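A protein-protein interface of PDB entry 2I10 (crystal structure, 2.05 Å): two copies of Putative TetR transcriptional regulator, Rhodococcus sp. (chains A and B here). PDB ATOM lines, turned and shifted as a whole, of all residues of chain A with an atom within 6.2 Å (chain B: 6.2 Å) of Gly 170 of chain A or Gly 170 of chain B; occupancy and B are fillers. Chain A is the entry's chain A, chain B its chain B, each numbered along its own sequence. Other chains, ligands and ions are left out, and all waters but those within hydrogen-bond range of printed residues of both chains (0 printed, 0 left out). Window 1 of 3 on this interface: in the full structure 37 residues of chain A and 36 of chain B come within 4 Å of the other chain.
CB of Met 165 of chain A touches OE2 of Glu 174 of chain B, at 3.5 Å.
CA of Gly 170 of chain B touches O of Ala 166 of chain A (3.0 Å).
CB of Ala 166 of chain A touches N of Leu 171 of chain B, at 3.8 Å.
Glu 174 of chain B touches Ala 166 of chain A (CG to N, 3.9 Å).
CG1 of Val 173 of chain B touches CG of Tyr 169 of chain A, at 3.7 Å.
Gly 170 of chain A touches Gly 170 of chain B.
Tyr 169 of chain B touches Val 173 of chain A.
OE1 of Glu 174 of chain A touches CE of Met 165 of chain B (3.5 Å).
CG of Glu 174 of chain A touches N of Ala 166 of chain B (3.95 Å).
CE2 of Tyr 169 of chain B touches OE1 of Glu 174 of chain A (3.2 Å).
Of chain B, only Ala 166 (3.1 Å) and Gly 170 (3.5 Å) come within 4 Å of Gly 170 of chain A.
Gly 170 of chain B touches two residues of chain A.
Printed residues of chain A within 4 Å of Ala 166 of chain B: Gly 170, Leu 171 and Glu 174.
Printed residues of chain B within 4 Å of Glu 174 of chain A: Met 165 (3.5 Å), Ala 166 (3.95 Å) and Tyr 169 (3.2 Å).
Of the printed residues of chain A, Met 165 of chain B touches Glu 174.
Of the printed residues of chain B, Leu 171 of chain A touches Ala 166 (3.9 Å).
The nearest residue of chain B that does not touch Gly 170 of chain A is Tyr 169 of chain B (4.3 Å).
Of the 13 printed residues of chain B, 7 touch a printed residue of chain A.
Of the 12 printed residues of chain A, 7 touch a printed residue of chain B.
Printed residues of chain A that touch a printed residue of chain B: Met 165, Ala 166, Tyr 169, Gly 170, Leu 171, Val 173 and Glu 174.
Hydrophobic or aromatic side chains of chain A that line the printed part of chain B: Met 165, Ala 166, Tyr 169, Leu 171 and Val 173.
Among the printed residues, 13 pairs touch across the chains.
Met 165 of chain A touches Glu 174 of chain B, and with the chains exchanged Glu 174 of chain A touches Met 165 of chain B.
Ala 166 of chain A touches Gly 170 of chain B, and with the chains exchanged Gly 170 of chain A touches Ala 166 of chain B.
Ala 166 of chain A touches Leu 171 of chain B, and with the chains exchanged Leu 171 of chain A touches Ala 166 of chain B.
Tyr 169 of chain A touches Glu 174 of chain B, and with the chains exchanged Glu 174 of chain A touches Tyr 169 of chain B.
Of the 13 pairs that touch across the chains among the printed residues, 13 have their exchanged pair printed and touching as well.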
ATOM      1  N   MET A 165      -6.832  -1.722  -9.435  1.00  0.00           N
ATOM      2  CA  MET A 165      -8.138  -2.278  -9.100  1.00  0.00           C
ATOM      3  C   MET A 165      -8.702  -3.145 -10.240  1.00  0.00           C
ATOM      4  O   MET A 165      -9.118  -4.288 -10.031  1.00  0.00           O
ATOM      5  CB  MET A 165      -9.108  -1.154  -8.759  1.00  0.00           C
ATOM      6  CG  MET A 165      -8.652  -0.315  -7.568  1.00  0.00           C
ATOM      7  SD  MET A 165      -8.532  -1.412  -5.952  1.00  0.00           S
ATOM      8  CE  MET A 165      -6.798  -2.307  -6.085  1.00  0.00           C
ATOM      9  N   ALA A 166      -8.700  -2.605 -11.445  1.00  0.00           N
ATOM     10  CA  ALA A 166      -9.175  -3.342 -12.622  1.00  0.00           C
ATOM     11  C   ALA A 166      -8.402  -4.652 -12.783  1.00  0.00           C
ATOM     12  O   ALA A 166      -8.997  -5.703 -12.994  1.00  0.00           O
ATOM     13  CB  ALA A 166      -9.015  -2.442 -13.868  1.00  0.00           C
ATOM     14  N   ALA A 167      -7.067  -4.605 -12.655  1.00  0.00           N
ATOM     15  CA  ALA A 167      -6.261  -5.813 -12.788  1.00  0.00           C
ATOM     16  C   ALA A 167      -6.677  -6.865 -11.747  1.00  0.00           C
ATOM     17  O   ALA A 167      -6.981  -8.009 -12.069  1.00  0.00           O
ATOM     18  CB  ALA A 167      -4.769  -5.519 -12.737  1.00  0.00           C
ATOM     19  N   VAL A 168      -6.778  -6.444 -10.506  1.00  0.00           N
ATOM     20  CA  VAL A 168      -7.092  -7.391  -9.453  1.00  0.00           C
ATOM     21  C   VAL A 168      -8.494  -8.021  -9.669  1.00  0.00           C
ATOM     22  O   VAL A 168      -8.678  -9.227  -9.554  1.00  0.00           O
ATOM     23  CB  VAL A 168      -6.848  -6.732  -8.032  1.00  0.00           C
ATOM     24  CG1 VAL A 168      -8.069  -6.079  -7.506  1.00  0.00           C
ATOM     25  CG2 VAL A 168      -6.364  -7.777  -7.058  1.00  0.00           C
ATOM     26  N   TYR A 169      -9.485  -7.212 -10.006  1.00  0.00           N
ATOM     27  CA  TYR A 169     -10.813  -7.768 -10.241  1.00  0.00           C
ATOM     28  C   TYR A 169     -10.879  -8.591 -11.549  1.00  0.00           C
ATOM     29  O   TYR A 169     -11.601  -9.578 -11.629  1.00  0.00           O
ATOM     30  CB  TYR A 169     -11.853  -6.655 -10.277  1.00  0.00           C
ATOM     31  CG  TYR A 169     -12.097  -5.981  -8.942  1.00  0.00           C
ATOM     32  CD1 TYR A 169     -12.747  -6.652  -7.888  1.00  0.00           C
ATOM     33  CD2 TYR A 169     -11.743  -4.669  -8.750  1.00  0.00           C
ATOM     34  CE1 TYR A 169     -13.019  -5.999  -6.658  1.00  0.00           C
ATOM     35  CE2 TYR A 169     -11.974  -4.007  -7.523  1.00  0.00           C
ATOM     36  CZ  TYR A 169     -12.608  -4.678  -6.487  1.00  0.00           C
ATOM     37  OH  TYR A 169     -12.844  -3.973  -5.296  1.00  0.00           O
ATOM     38  N   GLY A 170     -10.110  -8.193 -12.556  1.00  0.00           N
ATOM     39  CA  GLY A 170     -10.155  -8.888 -13.868  1.00  0.00           C
ATOM     40  C   GLY A 170      -9.505 -10.240 -13.720  1.00  0.00           C
ATOM     41  O   GLY A 170     -10.001 -11.240 -14.218  1.00  0.00           O
ATOM     42  N   LEU A 171      -8.401 -10.291 -12.976  1.00  0.00           N
ATOM     43  CA  LEU A 171      -7.746 -11.573 -12.712  1.00  0.00           C
ATOM     44  C   LEU A 171      -8.684 -12.467 -11.911  1.00  0.00           C
ATOM     45  O   LEU A 171      -8.680 -13.681 -12.050  1.00  0.00           O
ATOM     46  CB  LEU A 171      -6.413 -11.376 -11.945  1.00  0.00           C
ATOM     47  CG  LEU A 171      -5.246 -10.724 -12.696  1.00  0.00           C
ATOM     48  CD1 LEU A 171      -4.145 -10.189 -11.736  1.00  0.00           C
ATOM     49  CD2 LEU A 171      -4.652 -11.618 -13.800  1.00  0.00           C
ATOM     50  N   SER A 172      -9.481 -11.852 -11.056  1.00  0.00           N
ATOM     51  CA  SER A 172     -10.484 -12.549 -10.265  1.00  0.00           C
ATOM     52  C   SER A 172     -11.580 -13.175 -11.143  1.00  0.00           C
ATOM     53  O   SER A 172     -11.917 -14.350 -10.970  1.00  0.00           O
ATOM     54  CB  SER A 172     -11.080 -11.568  -9.246  1.00  0.00           C
ATOM     55  OG  SER A 172     -11.965 -12.234  -8.379  1.00  0.00           O
ATOM     56  N   VAL A 173     -12.118 -12.397 -12.083  1.00  0.00           N
ATOM     57  CA  VAL A 173     -13.074 -12.893 -13.103  1.00  0.00           C
ATOM     58  C   VAL A 173     -12.471 -14.025 -13.957  1.00  0.00           C
ATOM     59  O   VAL A 173     -13.120 -15.071 -14.124  1.00  0.00           O
ATOM     60  CB  VAL A 173     -13.591 -11.748 -14.033  1.00  0.00           C
ATOM     61  CG1 VAL A 173     -14.611 -12.270 -15.067  1.00  0.00           C
ATOM     62  CG2 VAL A 173     -14.206 -10.602 -13.232  1.00  0.00           C
ATOM     63  N   GLU A 174     -11.234 -13.847 -14.454  1.00  0.00           N
ATOM     64  CA  GLU A 174     -10.559 -14.900 -15.222  1.00  0.00           C
ATOM     65  C   GLU A 174     -10.449 -16.177 -14.460  1.00  0.00           C
ATOM     66  O   GLU A 174     -10.739 -17.238 -15.000  1.00  0.00           O
ATOM     67  CB  GLU A 174      -9.151 -14.502 -15.718  1.00  0.00           C
ATOM     68  CG  GLU A 174      -9.119 -13.931 -17.102  1.00  0.00           C
ATOM     69  CD  GLU A 174      -9.959 -14.785 -18.119  1.00  0.00           C
ATOM     70  OE1 GLU A 174     -10.934 -14.260 -18.598  1.00  0.00           O
ATOM     71  OE2 GLU A 174      -9.671 -15.981 -18.366  1.00  0.00           O
ATOM     72  N   ALA A 175     -10.017 -16.078 -13.197  1.00  0.00           N
ATOM     73  CA  ALA A 175      -9.893 -17.233 -12.320  1.00  0.00           C
ATOM     74  C   ALA A 175     -11.235 -17.913 -12.063  1.00  0.00           C
ATOM     75  O   ALA A 175     -11.321 -19.159 -12.077  1.00  0.00           O
ATOM     76  CB  ALA A 175      -9.235 -16.829 -10.982  1.00  0.00           C
ATOM     77  N   LEU A 184      -2.589 -17.355 -15.327  1.00  0.00           N
ATOM     78  CA  LEU A 184      -2.990 -16.254 -14.449  1.00  0.00           C
ATOM     79  C   LEU A 184      -1.817 -15.656 -13.694  1.00  0.00           C
ATOM     80  O   LEU A 184      -1.770 -14.446 -13.468  1.00  0.00           O
ATOM     81  CB  LEU A 184      -4.030 -16.732 -13.448  1.00  0.00           C
ATOM     82  CG  LEU A 184      -5.474 -16.822 -13.912  1.00  0.00           C
ATOM     83  CD1 LEU A 184      -6.224 -17.526 -12.810  1.00  0.00           C
ATOM     84  CD2 LEU A 184      -6.058 -15.441 -14.124  1.00  0.00           C
ATOM     85  N   VAL B 110     -18.682 -11.109 -16.302  1.00  0.00           N
ATOM     86  CA  VAL B 110     -18.571 -10.705 -14.906  1.00  0.00           C
ATOM     87  C   VAL B 110     -19.746 -11.319 -14.107  1.00  0.00           C
ATOM     88  O   VAL B 110     -19.525 -12.024 -13.129  1.00  0.00           O
ATOM     89  CB  VAL B 110     -18.486  -9.160 -14.734  1.00  0.00           C
ATOM     90  CG1 VAL B 110     -18.760  -8.751 -13.282  1.00  0.00           C
ATOM     91  CG2 VAL B 110     -17.094  -8.631 -15.204  1.00  0.00           C
ATOM     92  N   MET B 165      -7.657 -10.263 -21.516  1.00  0.00           N
ATOM     93  CA  MET B 165      -8.975 -10.685 -21.069  1.00  0.00           C
ATOM     94  C   MET B 165      -9.253 -10.200 -19.634  1.00  0.00           C
ATOM     95  O   MET B 165     -10.319  -9.681 -19.338  1.00  0.00           O
ATOM     96  CB  MET B 165      -9.063 -12.205 -21.121  1.00  0.00           C
ATOM     97  CG  MET B 165      -8.982 -12.824 -22.590  1.00  0.00           C
ATOM     98  SD  MET B 165      -8.772 -14.750 -22.457  1.00  0.00           S
ATOM     99  CE  MET B 165     -10.551 -15.296 -21.890  1.00  0.00           C
ATOM    100  N   ALA B 166      -8.297 -10.429 -18.737  1.00  0.00           N
ATOM    101  CA  ALA B 166      -8.339  -9.868 -17.366  1.00  0.00           C
ATOM    102  C   ALA B 166      -8.517  -8.350 -17.381  1.00  0.00           C
ATOM    103  O   ALA B 166      -9.369  -7.802 -16.667  1.00  0.00           O
ATOM    104  CB  ALA B 166      -7.066 -10.281 -16.597  1.00  0.00           C
ATOM    105  N   ALA B 167      -7.789  -7.656 -18.250  1.00  0.00           N
ATOM    106  CA  ALA B 167      -7.953  -6.208 -18.315  1.00  0.00           C
ATOM    107  C   ALA B 167      -9.386  -5.761 -18.719  1.00  0.00           C
ATOM    108  O   ALA B 167      -9.962  -4.857 -18.103  1.00  0.00           O
ATOM    109  CB  ALA B 167      -6.879  -5.554 -19.230  1.00  0.00           C
ATOM    110  N   VAL B 168      -9.983  -6.398 -19.728  1.00  0.00           N
ATOM    111  CA  VAL B 168     -11.332  -6.053 -20.171  1.00  0.00           C
ATOM    112  C   VAL B 168     -12.365  -6.244 -19.075  1.00  0.00           C
ATOM    113  O   VAL B 168     -13.220  -5.415 -18.857  1.00  0.00           O
ATOM    114  CB  VAL B 168     -11.824  -6.957 -21.366  1.00  0.00           C
ATOM    115  CG1 VAL B 168     -13.276  -6.654 -21.697  1.00  0.00           C
ATOM    116  CG2 VAL B 168     -10.983  -6.757 -22.588  1.00  0.00           C
ATOM    117  N   TYR B 169     -12.331  -7.430 -18.453  1.00  0.00           N
ATOM    118  CA  TYR B 169     -13.289  -7.743 -17.404  1.00  0.00           C
ATOM    119  C   TYR B 169     -13.083  -6.842 -16.181  1.00  0.00           C
ATOM    120  O   TYR B 169     -14.039  -6.428 -15.571  1.00  0.00           O
ATOM    121  CB  TYR B 169     -13.163  -9.193 -17.017  1.00  0.00           C
ATOM    122  CG  TYR B 169     -13.478 -10.125 -18.152  1.00  0.00           C
ATOM    123  CD1 TYR B 169     -14.690 -10.024 -18.850  1.00  0.00           C
ATOM    124  CD2 TYR B 169     -12.568 -11.104 -18.546  1.00  0.00           C
ATOM    125  CE1 TYR B 169     -14.986 -10.902 -19.910  1.00  0.00           C
ATOM    126  CE2 TYR B 169     -12.865 -11.980 -19.615  1.00  0.00           C
ATOM    127  CZ  TYR B 169     -14.058 -11.864 -20.286  1.00  0.00           C
ATOM    128  OH  TYR B 169     -14.366 -12.756 -21.316  1.00  0.00           O
ATOM    129  N   GLY B 170     -11.829  -6.538 -15.851  1.00  0.00           N
ATOM    130  CA  GLY B 170     -11.522  -5.636 -14.703  1.00  0.00           C
ATOM    131  C   GLY B 170     -12.001  -4.226 -14.938  1.00  0.00           C
ATOM    132  O   GLY B 170     -12.562  -3.574 -14.015  1.00  0.00           O
ATOM    133  N   LEU B 171     -11.786  -3.725 -16.157  1.00  0.00           N
ATOM    134  CA  LEU B 171     -12.355  -2.402 -16.506  1.00  0.00           C
ATOM    135  C   LEU B 171     -13.880  -2.418 -16.460  1.00  0.00           C
ATOM    136  O   LEU B 171     -14.479  -1.451 -16.019  1.00  0.00           O
ATOM    137  CB  LEU B 171     -11.876  -1.918 -17.868  1.00  0.00           C
ATOM    138  CG  LEU B 171     -10.401  -1.539 -17.954  1.00  0.00           C
ATOM    139  CD1 LEU B 171      -9.941  -1.671 -19.429  1.00  0.00           C
ATOM    140  CD2 LEU B 171     -10.219  -0.131 -17.467  1.00  0.00           C
ATOM    141  N   SER B 172     -14.506  -3.537 -16.864  1.00  0.00           N
ATOM    142  CA  SER B 172     -15.977  -3.667 -16.756  1.00  0.00           C
ATOM    143  C   SER B 172     -16.456  -3.570 -15.293  1.00  0.00           C
ATOM    144  O   SER B 172     -17.462  -2.906 -14.975  1.00  0.00           O
ATOM    145  CB  SER B 172     -16.447  -5.021 -17.338  1.00  0.00           C
ATOM    146  OG  SER B 172     -17.794  -5.260 -16.987  1.00  0.00           O
ATOM    147  N   VAL B 173     -15.762  -4.293 -14.425  1.00  0.00           N
ATOM    148  CA  VAL B 173     -16.058  -4.263 -12.984  1.00  0.00           C
ATOM    149  C   VAL B 173     -15.949  -2.828 -12.407  1.00  0.00           C
ATOM    150  O   VAL B 173     -16.832  -2.379 -11.696  1.00  0.00           O
ATOM    151  CB  VAL B 173     -15.142  -5.250 -12.182  1.00  0.00           C
ATOM    152  CG1 VAL B 173     -15.178  -4.895 -10.637  1.00  0.00           C
ATOM    153  CG2 VAL B 173     -15.592  -6.666 -12.437  1.00  0.00           C
ATOM    154  N   GLU B 174     -14.892  -2.115 -12.758  1.00  0.00           N
ATOM    155  CA  GLU B 174     -14.707  -0.771 -12.283  1.00  0.00           C
ATOM    156  C   GLU B 174     -15.786   0.162 -12.796  1.00  0.00           C
ATOM    157  O   GLU B 174     -16.318   0.951 -12.040  1.00  0.00           O
ATOM    158  CB  GLU B 174     -13.275  -0.271 -12.574  1.00  0.00           C
ATOM    159  CG  GLU B 174     -12.228  -0.999 -11.720  1.00  0.00           C
ATOM    160  CD  GLU B 174     -12.470  -0.764 -10.245  1.00  0.00           C
ATOM    161  OE1 GLU B 174     -12.742   0.382  -9.830  1.00  0.00           O
ATOM    162  OE2 GLU B 174     -12.456  -1.734  -9.508  1.00  0.00           O
ATOM    163  N   ALA B 175     -16.138   0.036 -14.083  1.00  0.00           N
ATOM    164  CA  ALA B 175     -17.228   0.813 -14.664  1.00  0.00           C
ATOM    165  C   ALA B 175     -18.557   0.576 -13.945  1.00  0.00           C
ATOM    166  O   ALA B 175     -19.279   1.529 -13.620  1.00  0.00           O
ATOM    167  CB  ALA B 175     -17.346   0.471 -16.174  1.00  0.00           C
ATOM    168  N   LEU B 184     -11.274   5.953 -15.921  1.00  0.00           N
ATOM    169  CA  LEU B 184     -11.272   4.586 -16.451  1.00  0.00           C
ATOM    170  C   LEU B 184     -10.579   4.508 -17.816  1.00  0.00           C
ATOM    171  O   LEU B 184      -9.874   3.536 -18.121  1.00  0.00           O
ATOM    172  CB  LEU B 184     -12.697   3.994 -16.508  1.00  0.00           C
ATOM    173  CG  LEU B 184     -12.758   2.481 -16.315  1.00  0.00           C
ATOM    174  CD1 LEU B 184     -12.010   2.035 -15.053  1.00  0.00           C
ATOM    175  CD2 LEU B 184     -14.188   1.956 -16.306  1.00  0.00           C
